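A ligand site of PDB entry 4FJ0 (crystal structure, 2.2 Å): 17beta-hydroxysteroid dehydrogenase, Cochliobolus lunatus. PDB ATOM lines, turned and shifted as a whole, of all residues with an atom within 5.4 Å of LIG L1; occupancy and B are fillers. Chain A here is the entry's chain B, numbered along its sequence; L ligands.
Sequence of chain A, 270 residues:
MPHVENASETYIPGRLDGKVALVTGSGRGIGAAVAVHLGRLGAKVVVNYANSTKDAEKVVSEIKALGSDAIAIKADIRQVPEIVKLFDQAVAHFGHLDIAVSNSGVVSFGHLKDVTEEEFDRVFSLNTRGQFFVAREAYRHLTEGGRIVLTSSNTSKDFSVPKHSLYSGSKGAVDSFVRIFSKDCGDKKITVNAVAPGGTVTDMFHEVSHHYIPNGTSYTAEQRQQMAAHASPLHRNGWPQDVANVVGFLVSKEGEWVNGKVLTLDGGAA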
ATOM      1  N   VAL A 107     -26.180   5.988   1.596  1.00  0.00           N
ATOM      2  CA  VAL A 107     -27.252   5.161   1.070  1.00  0.00           C
ATOM      3  C   VAL A 107     -27.384   3.928   1.976  1.00  0.00           C
ATOM      4  O   VAL A 107     -26.500   3.617   2.744  1.00  0.00           O
ATOM      5  CB  VAL A 107     -26.953   4.714  -0.394  1.00  0.00           C
ATOM      6  CG1 VAL A 107     -25.865   3.630  -0.451  1.00  0.00           C
ATOM      7  CG2 VAL A 107     -28.221   4.195  -1.062  1.00  0.00           C
ATOM      8  N   SER A 153     -33.359  12.858  -3.647  1.00  0.00           N
ATOM      9  CA  SER A 153     -33.137  11.719  -4.513  1.00  0.00           C
ATOM     10  C   SER A 153     -34.395  11.449  -5.305  1.00  0.00           C
ATOM     11  O   SER A 153     -35.483  11.674  -4.816  1.00  0.00           O
ATOM     12  CB  SER A 153     -32.817  10.506  -3.619  1.00  0.00           C
ATOM     13  OG  SER A 153     -32.835   9.300  -4.337  1.00  0.00           O
ATOM     14  N   ASN A 154     -34.264  10.875  -6.488  1.00  0.00           N
ATOM     15  CA  ASN A 154     -35.446  10.462  -7.230  1.00  0.00           C
ATOM     16  C   ASN A 154     -36.252   9.388  -6.485  1.00  0.00           C
ATOM     17  O   ASN A 154     -37.446   9.231  -6.745  1.00  0.00           O
ATOM     18  CB  ASN A 154     -35.118  10.026  -8.673  1.00  0.00           C
ATOM     19  CG  ASN A 154     -34.277   8.769  -8.755  1.00  0.00           C
ATOM     20  OD1 ASN A 154     -33.628   8.337  -7.777  1.00  0.00           O
ATOM     21  ND2 ASN A 154     -34.219   8.202  -9.965  1.00  0.00           N
ATOM     22  N   THR A 155     -35.607   8.674  -5.558  1.00  0.00           N
ATOM     23  CA  THR A 155     -36.288   7.610  -4.779  1.00  0.00           C
ATOM     24  C   THR A 155     -37.263   8.124  -3.712  1.00  0.00           C
ATOM     25  O   THR A 155     -38.077   7.373  -3.190  1.00  0.00           O
ATOM     26  CB  THR A 155     -35.282   6.697  -4.067  1.00  0.00           C
ATOM     27  OG1 THR A 155     -34.498   7.486  -3.179  1.00  0.00           O
ATOM     28  CG2 THR A 155     -34.360   6.002  -5.108  1.00  0.00           C
ATOM     29  N   PHE A 159     -39.335   7.229  -7.895  1.00  0.00           N
ATOM     30  CA  PHE A 159     -38.762   5.930  -8.234  1.00  0.00           C
ATOM     31  C   PHE A 159     -38.894   5.045  -7.010  1.00  0.00           C
ATOM     32  O   PHE A 159     -38.495   5.448  -5.923  1.00  0.00           O
ATOM     33  CB  PHE A 159     -37.303   6.177  -8.620  1.00  0.00           C
ATOM     34  CG  PHE A 159     -36.570   4.976  -9.137  1.00  0.00           C
ATOM     35  CD1 PHE A 159     -37.145   4.114 -10.047  1.00  0.00           C
ATOM     36  CD2 PHE A 159     -35.248   4.750  -8.736  1.00  0.00           C
ATOM     37  CE1 PHE A 159     -36.446   3.014 -10.503  1.00  0.00           C
ATOM     38  CE2 PHE A 159     -34.533   3.650  -9.208  1.00  0.00           C
ATOM     39  CZ  PHE A 159     -35.142   2.778 -10.095  1.00  0.00           C
ATOM     40  N   HIS A 164     -35.740  -0.189   0.149  1.00  0.00           N
ATOM     41  CA  HIS A 164     -35.088   1.109   0.104  1.00  0.00           C
ATOM     42  C   HIS A 164     -35.850   2.126   0.897  1.00  0.00           C
ATOM     43  O   HIS A 164     -35.777   3.316   0.612  1.00  0.00           O
ATOM     44  CB  HIS A 164     -34.983   1.522  -1.352  1.00  0.00           C
ATOM     45  CG  HIS A 164     -33.856   2.462  -1.657  1.00  0.00           C
ATOM     46  ND1 HIS A 164     -32.695   2.452  -0.985  1.00  0.00           N
ATOM     47  CD2 HIS A 164     -33.707   3.382  -2.673  1.00  0.00           C
ATOM     48  CE1 HIS A 164     -31.876   3.388  -1.499  1.00  0.00           C
ATOM     49  NE2 HIS A 164     -32.485   3.958  -2.539  1.00  0.00           N
ATOM     50  N   TYR A 167     -33.773   5.006   3.224  1.00  0.00           N
ATOM     51  CA  TYR A 167     -33.164   6.047   2.419  1.00  0.00           C
ATOM     52  C   TYR A 167     -34.209   6.910   1.744  1.00  0.00           C
ATOM     53  O   TYR A 167     -34.088   8.140   1.717  1.00  0.00           O
ATOM     54  CB  TYR A 167     -32.270   5.414   1.351  1.00  0.00           C
ATOM     55  CG  TYR A 167     -31.561   6.415   0.470  1.00  0.00           C
ATOM     56  CD1 TYR A 167     -30.441   7.097   0.925  1.00  0.00           C
ATOM     57  CD2 TYR A 167     -32.033   6.704  -0.802  1.00  0.00           C
ATOM     58  CE1 TYR A 167     -29.759   8.002   0.107  1.00  0.00           C
ATOM     59  CE2 TYR A 167     -31.389   7.592  -1.620  1.00  0.00           C
ATOM     60  CZ  TYR A 167     -30.250   8.254  -1.170  1.00  0.00           C
ATOM     61  OH  TYR A 167     -29.611   9.164  -2.012  1.00  0.00           O
ATOM     62  N   PRO A 197     -31.194  13.780  -7.614  1.00  0.00           N
ATOM     63  CA  PRO A 197     -30.641  13.015  -8.712  1.00  0.00           C
ATOM     64  C   PRO A 197     -31.160  11.600  -8.755  1.00  0.00           C
ATOM     65  O   PRO A 197     -31.513  11.053  -7.722  1.00  0.00           O
ATOM     66  CB  PRO A 197     -29.131  12.980  -8.407  1.00  0.00           C
ATOM     67  CG  PRO A 197     -28.912  14.045  -7.376  1.00  0.00           C
ATOM     68  CD  PRO A 197     -30.184  14.115  -6.602  1.00  0.00           C
ATOM     69  N   GLY A 198     -31.196  11.028  -9.950  1.00  0.00           N
ATOM     70  CA  GLY A 198     -31.315   9.579 -10.090  1.00  0.00           C
ATOM     71  C   GLY A 198     -29.922   8.996 -10.053  1.00  0.00           C
ATOM     72  O   GLY A 198     -29.001   9.618  -9.539  1.00  0.00           O
ATOM     73  N   GLY A 199     -29.756   7.796 -10.599  1.00  0.00           N
ATOM     74  CA  GLY A 199     -28.478   7.132 -10.595  1.00  0.00           C
ATOM     75  C   GLY A 199     -27.428   7.974 -11.290  1.00  0.00           C
ATOM     76  O   GLY A 199     -27.536   8.262 -12.453  1.00  0.00           O
ATOM     77  N   THR A 200     -26.404   8.347 -10.525  1.00  0.00           N
ATOM     78  CA  THR A 200     -25.330   9.184 -10.991  1.00  0.00           C
ATOM     79  C   THR A 200     -24.035   8.455 -10.654  1.00  0.00           C
ATOM     80  O   THR A 200     -23.846   8.011  -9.517  1.00  0.00           O
ATOM     81  CB  THR A 200     -25.387  10.539 -10.242  1.00  0.00           C
ATOM     82  OG1 THR A 200     -26.698  11.118 -10.369  1.00  0.00           O
ATOM     83  CG2 THR A 200     -24.303  11.517 -10.774  1.00  0.00           C
ATOM     84  N   MET A 204     -20.789   5.846  -4.647  1.00  0.00           N
ATOM     85  CA  MET A 204     -22.070   5.340  -4.137  1.00  0.00           C
ATOM     86  C   MET A 204     -22.798   4.493  -5.188  1.00  0.00           C
ATOM     87  O   MET A 204     -23.462   3.499  -4.847  1.00  0.00           O
ATOM     88  CB  MET A 204     -22.980   6.505  -3.704  1.00  0.00           C
ATOM     89  CG  MET A 204     -24.349   6.090  -3.180  1.00  0.00           C
ATOM     90  SD  MET A 204     -25.454   7.477  -2.770  1.00  0.00           S
ATOM     91  CE  MET A 204     -24.616   8.169  -1.326  1.00  0.00           C
ATOM     92  N   PHE A 205     -22.723   4.919  -6.450  1.00  0.00           N
ATOM     93  CA  PHE A 205     -23.412   4.236  -7.514  1.00  0.00           C
ATOM     94  C   PHE A 205     -22.928   2.800  -7.590  1.00  0.00           C
ATOM     95  O   PHE A 205     -23.713   1.862  -7.559  1.00  0.00           O
ATOM     96  CB  PHE A 205     -23.132   4.904  -8.849  1.00  0.00           C
ATOM     97  CG  PHE A 205     -23.812   4.246  -9.967  1.00  0.00           C
ATOM     98  CD1 PHE A 205     -23.215   3.168 -10.590  1.00  0.00           C
ATOM     99  CD2 PHE A 205     -25.055   4.683 -10.406  1.00  0.00           C
ATOM    100  CE1 PHE A 205     -23.835   2.541 -11.621  1.00  0.00           C
ATOM    101  CE2 PHE A 205     -25.690   4.058 -11.457  1.00  0.00           C
ATOM    102  CZ  PHE A 205     -25.071   2.985 -12.059  1.00  0.00           C
ATOM    103  N   HIS A 206     -21.620   2.656  -7.707  1.00  0.00           N
ATOM    104  CA  HIS A 206     -21.013   1.342  -7.821  1.00  0.00           C
ATOM    105  C   HIS A 206     -21.158   0.513  -6.591  1.00  0.00           C
ATOM    106  O   HIS A 206     -21.231  -0.699  -6.666  1.00  0.00           O
ATOM    107  CB  HIS A 206     -19.552   1.473  -8.217  1.00  0.00           C
ATOM    108  CG  HIS A 206     -19.340   2.028  -9.596  1.00  0.00           C
ATOM    109  ND1 HIS A 206     -18.784   3.254  -9.814  1.00  0.00           N
ATOM    110  CD2 HIS A 206     -19.649   1.503 -10.863  1.00  0.00           C
ATOM    111  CE1 HIS A 206     -18.731   3.477 -11.144  1.00  0.00           C
ATOM    112  NE2 HIS A 206     -19.260   2.408 -11.789  1.00  0.00           N
ATOM    113  N   VAL A 208     -23.805   0.333  -4.686  1.00  0.00           N
ATOM    114  CA  VAL A 208     -25.193  -0.170  -4.527  1.00  0.00           C
ATOM    115  C   VAL A 208     -26.020  -0.483  -5.792  1.00  0.00           C
ATOM    116  O   VAL A 208     -27.149  -0.949  -5.687  1.00  0.00           O
ATOM    117  CB  VAL A 208     -25.963   0.768  -3.597  1.00  0.00           C
ATOM    118  CG1 VAL A 208     -25.199   0.850  -2.278  1.00  0.00           C
ATOM    119  CG2 VAL A 208     -26.142   2.143  -4.239  1.00  0.00           C
ATOM    120  N   SER A 209     -25.444  -0.317  -6.984  1.00  0.00           N
ATOM    121  CA  SER A 209     -26.196  -0.551  -8.233  1.00  0.00           C
ATOM    122  C   SER A 209     -26.881  -1.936  -8.274  1.00  0.00           C
ATOM    123  O   SER A 209     -27.921  -2.075  -8.895  1.00  0.00           O
ATOM    124  CB  SER A 209     -25.285  -0.341  -9.456  1.00  0.00           C
ATOM    125  OG  SER A 209     -24.239  -1.284  -9.451  1.00  0.00           O
ATOM    126  N   TYR A 212     -30.584  -2.017  -7.157  1.00  0.00           N
ATOM    127  CA  TYR A 212     -31.561  -1.379  -8.038  1.00  0.00           C
ATOM    128  C   TYR A 212     -32.017  -2.272  -9.162  1.00  0.00           C
ATOM    129  O   TYR A 212     -32.999  -1.957  -9.825  1.00  0.00           O
ATOM    130  CB  TYR A 212     -31.005  -0.061  -8.591  1.00  0.00           C
ATOM    131  CG  TYR A 212     -30.829   0.988  -7.516  1.00  0.00           C
ATOM    132  CD1 TYR A 212     -31.883   1.824  -7.231  1.00  0.00           C
ATOM    133  CD2 TYR A 212     -29.635   1.141  -6.778  1.00  0.00           C
ATOM    134  CE1 TYR A 212     -31.802   2.793  -6.264  1.00  0.00           C
ATOM    135  CE2 TYR A 212     -29.535   2.147  -5.805  1.00  0.00           C
ATOM    136  CZ  TYR A 212     -30.633   2.961  -5.556  1.00  0.00           C
ATOM    137  OH  TYR A 212     -30.606   3.959  -4.592  1.00  0.00           O
ATOM    138  N   ILE A 213     -31.327  -3.387  -9.366  1.00  0.00           N
ATOM    139  CA  ILE A 213     -31.597  -4.276 -10.472  1.00  0.00           C
ATOM    140  C   ILE A 213     -32.015  -5.676  -9.970  1.00  0.00           C
ATOM    141  O   ILE A 213     -31.377  -6.234  -9.076  1.00  0.00           O
ATOM    142  CB  ILE A 213     -30.340  -4.450 -11.352  1.00  0.00           C
ATOM    143  CG1 ILE A 213     -29.946  -3.112 -11.994  1.00  0.00           C
ATOM    144  CG2 ILE A 213     -30.579  -5.506 -12.408  1.00  0.00           C
ATOM    145  CD1 ILE A 213     -28.597  -3.141 -12.687  1.00  0.00           C
ATOM    146  N   ARG A 224     -24.197  -3.341 -14.999  1.00  0.00           N
ATOM    147  CA  ARG A 224     -25.178  -2.681 -14.162  1.00  0.00           C
ATOM    148  C   ARG A 224     -25.242  -1.196 -14.496  1.00  0.00           C
ATOM    149  O   ARG A 224     -26.320  -0.609 -14.536  1.00  0.00           O
ATOM    150  CB  ARG A 224     -24.862  -2.914 -12.682  1.00  0.00           C
ATOM    151  CG  ARG A 224     -25.210  -4.316 -12.181  1.00  0.00           C
ATOM    152  CD  ARG A 224     -25.290  -4.366 -10.675  1.00  0.00           C
ATOM    153  NE  ARG A 224     -24.014  -4.025 -10.058  1.00  0.00           N
ATOM    154  CZ  ARG A 224     -23.008  -4.873  -9.862  1.00  0.00           C
ATOM    155  NH1 ARG A 224     -23.097  -6.142 -10.230  1.00  0.00           N
ATOM    156  NH2 ARG A 224     -21.889  -4.434  -9.304  1.00  0.00           N
ATOM    157  N   MET A 227     -27.126  -0.742 -17.688  1.00  0.00           N
ATOM    158  CA  MET A 227     -28.587  -0.822 -17.492  1.00  0.00           C
ATOM    159  C   MET A 227     -29.162   0.455 -16.918  1.00  0.00           C
ATOM    160  O   MET A 227     -30.253   0.873 -17.310  1.00  0.00           O
ATOM    161  CB  MET A 227     -28.959  -2.030 -16.644  1.00  0.00           C
ATOM    162  CG  MET A 227     -28.854  -3.331 -17.415  1.00  0.00           C
ATOM    163  SD  MET A 227     -28.913  -4.760 -16.332  1.00  0.00           S
ATOM    164  CE  MET A 227     -30.347  -4.309 -15.334  1.00  0.00           C
ATOM    165  N   ALA A 228     -28.442   1.090 -15.997  1.00  0.00           N
ATOM    166  CA  ALA A 228     -28.840   2.406 -15.483  1.00  0.00           C
ATOM    167  C   ALA A 228     -28.862   3.445 -16.610  1.00  0.00           C
ATOM    168  O   ALA A 228     -29.723   4.311 -16.635  1.00  0.00           O
ATOM    169  CB  ALA A 228     -27.960   2.863 -14.325  1.00  0.00           C
HETATM  170  C1  LIG L   1     -30.398   2.773 -10.710  1.00  0.00           C
HETATM  171  C2  LIG L   1     -30.748   1.922 -11.764  1.00  0.00           C
HETATM  172  C3  LIG L   1     -29.866   0.949 -12.220  1.00  0.00           C
HETATM  173  C4  LIG L   1     -28.615   0.839 -11.628  1.00  0.00           C
HETATM  174  C5  LIG L   1     -28.261   1.716 -10.584  1.00  0.00           C
HETATM  175  C6  LIG L   1     -29.133   2.706 -10.119  1.00  0.00           C
HETATM  176  C7  LIG L   1     -28.829   3.574  -9.035  1.00  0.00           C
HETATM  177  O1  LIG L   1     -29.798   4.480  -8.737  1.00  0.00           O
HETATM  178  C8  LIG L   1     -29.674   5.292  -7.683  1.00  0.00           C
HETATM  179  C9  LIG L   1     -30.733   6.167  -7.441  1.00  0.00           C
HETATM  180  C10 LIG L   1     -30.659   7.030  -6.349  1.00  0.00           C
HETATM  181  O2  LIG L   1     -31.677   7.905  -6.111  1.00  0.00           O
HETATM  182  C11 LIG L   1     -29.528   7.021  -5.515  1.00  0.00           C
HETATM  183  C12 LIG L   1     -28.467   6.130  -5.761  1.00  0.00           C
HETATM  184  C13 LIG L   1     -28.551   5.280  -6.863  1.00  0.00           C
HETATM  185  C14 LIG L   1     -27.520   4.380  -7.144  1.00  0.00           C
HETATM  186  O3  LIG L   1     -26.505   4.318  -6.440  1.00  0.00           O
HETATM  187  C15 LIG L   1     -27.695   3.508  -8.234  1.00  0.00           C
HETATM  188  O4  LIG L   1     -26.703   2.632  -8.485  1.00  0.00           O
HETATM  189  P1  LG2 L   2     -20.629   9.302  -2.423  1.00  0.00           P
HETATM  190  O1  LG2 L   2     -20.734   8.195  -1.450  1.00  0.00           O
HETATM  191  O2  LG2 L   2     -19.779   9.181  -3.621  1.00  0.00           O
HETATM  192  O3  LG2 L   2     -20.127  10.602  -1.626  1.00  0.00           O
HETATM  193  C1  LG2 L   2     -20.619  10.908  -0.353  1.00  0.00           C
HETATM  194  C2  LG2 L   2     -20.131  12.283   0.120  1.00  0.00           C
HETATM  195  O4  LG2 L   2     -20.748  12.470   1.417  1.00  0.00           O
HETATM  196  C3  LG2 L   2     -18.617  12.339   0.342  1.00  0.00           C
HETATM  197  O5  LG2 L   2     -18.132  13.653   0.005  1.00  0.00           O
HETATM  198  C4  LG2 L   2     -18.481  12.104   1.854  1.00  0.00           C
HETATM  199  O6  LG2 L   2     -17.354  12.793   2.310  1.00  0.00           O
HETATM  200  C5  LG2 L   2     -19.703  12.817   2.370  1.00  0.00           C
HETATM  201  N1  LG2 L   2     -19.943  12.349   3.770  1.00  0.00           N
HETATM  202  C6  LG2 L   2     -20.132  11.091   4.206  1.00  0.00           C
HETATM  203  N2  LG2 L   2     -20.276  11.127   5.526  1.00  0.00           N
HETATM  204  C7  LG2 L   2     -20.177  12.378   5.954  1.00  0.00           C
HETATM  205  C8  LG2 L   2     -20.256  12.993   7.206  1.00  0.00           C
HETATM  206  N3  LG2 L   2     -20.445  12.282   8.305  1.00  0.00           N
HETATM  207  N4  LG2 L   2     -20.102  14.323   7.282  1.00  0.00           N
HETATM  208  C9  LG2 L   2     -19.892  15.028   6.173  1.00  0.00           C
HETATM  209  N5  LG2 L   2     -19.818  14.487   4.959  1.00  0.00           N
HETATM  210  C10 LG2 L   2     -19.955  13.159   4.830  1.00  0.00           C
HETATM  211  O7  LG2 L   2     -22.116   9.742  -2.792  1.00  0.00           O
HETATM  212  P2  LG2 L   2     -22.602  10.781  -3.981  1.00  0.00           P
HETATM  213  O8  LG2 L   2     -21.577  11.848  -4.198  1.00  0.00           O
HETATM  214  O9  LG2 L   2     -23.028   9.975  -5.126  1.00  0.00           O
HETATM  215  O10 LG2 L   2     -23.875  11.291  -3.226  1.00  0.00           O
HETATM  216  C11 LG2 L   2     -23.931  12.641  -2.725  1.00  0.00           C
HETATM  217  C12 LG2 L   2     -25.387  13.027  -2.448  1.00  0.00           C
HETATM  218  O11 LG2 L   2     -26.231  12.662  -3.592  1.00  0.00           O
HETATM  219  C13 LG2 L   2     -25.890  12.216  -1.259  1.00  0.00           C
HETATM  220  O12 LG2 L   2     -26.757  13.069  -0.496  1.00  0.00           O
HETATM  221  C14 LG2 L   2     -26.694  11.104  -1.914  1.00  0.00           C
HETATM  222  O13 LG2 L   2     -27.762  10.642  -1.031  1.00  0.00           O
HETATM  223  C15 LG2 L   2     -27.313  11.859  -3.097  1.00  0.00           C
HETATM  224  N6  LG2 L   2     -27.709  11.039  -4.270  1.00  0.00           N
HETATM  225  C16 LG2 L   2     -26.739  10.291  -4.978  1.00  0.00           C
HETATM  226  C17 LG2 L   2     -27.119   9.504  -6.074  1.00  0.00           C
HETATM  227  C18 LG2 L   2     -26.094   8.695  -6.909  1.00  0.00           C
HETATM  228  O14 LG2 L   2     -26.527   7.867  -7.906  1.00  0.00           O
HETATM  229  N7  LG2 L   2     -24.794   8.970  -6.765  1.00  0.00           N
HETATM  230  C19 LG2 L   2     -28.468   9.493  -6.448  1.00  0.00           C
HETATM  231  C20 LG2 L   2     -29.412  10.229  -5.745  1.00  0.00           C
HETATM  232  C21 LG2 L   2     -29.031  10.986  -4.648  1.00  0.00           C
HETATM  233  P3  LG2 L   2     -16.138  12.038   3.012  1.00  0.00           P
HETATM  234  O15 LG2 L   2     -15.067  12.985   3.367  1.00  0.00           O
HETATM  235  O16 LG2 L   2     -15.658  10.974   2.027  1.00  0.00           O
HETATM  236  O17 LG2 L   2     -16.755  11.326   4.270  1.00  0.00           O
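The side-chain hydroxyl (OG1) of Thr 155 sits at hydrogen-bond distance from the side-chain hydroxyl (OG) of Ser 153, at 2.7 Å.
The backbone carbonyl oxygen of Pro 197 sits at hydrogen-bond distance from the backbone NH of Asn 154 (3.0 Å).
O of Asn 154 is in hydrogen-bond range of N of Phe 159, at 3.0 Å.
OG of Ser 209 is in hydrogen-bond range of NE of Arg 224, at 2.8 Å.
NE2 of His 164 is in hydrogen-bond range of OH of Tyr 212 (2.8 Å).
The side-chain hydroxyl of Thr 200 is in hydrogen-bond range of the backbone carbonyl oxygen of Gly 198 (2.9 Å).
Merely in contact with LIG L1: Val 208, Ser 209, Tyr 212, Ala 228, Thr 155, Gly 199, Met 204, Pro 197, Gly 198 and Arg 224.
Hydrophobic or aromatic side chains within 4 Å of LIG L1: Phe 205, Val 208, Tyr 212 and Ala 228.
Of the 21 residues printed, 13 come within 4 Å of LIG L1.
Along chain A the residues within 4 Å of LIG L1 span positions 153 to 228.
The nearest printed residue that does not touch LIG L1 is Ile 213 (4.1 Å).
The side-chain hydroxyl (OG) of Ser 153 sits at hydrogen-bond distance from an oxygen (O2) of LIG L1 (2.5 Å).
O2 of LIG L1 lies within hydrogen-bond range of OD1 of Asn 154, at 2.6 Å.
The backbone carbonyl oxygen of Phe 205 lies within hydrogen-bond range of an oxygen (O4) of LIG L1, at 3.2 Å.
The side-chain hydroxyl of Tyr 167 is in hydrogen-bond range of an oxygen (O13) of LG2 L2.
The backbone NH (N) of Thr 200 sits at hydrogen-bond distance from an oxygen (O14) of LG2 L2 (2.7 Å).
The backbone carbonyl oxygen of Thr 200 lies within hydrogen-bond range of a nitrogen (N7) of LG2 L2, at 3.1 Å.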
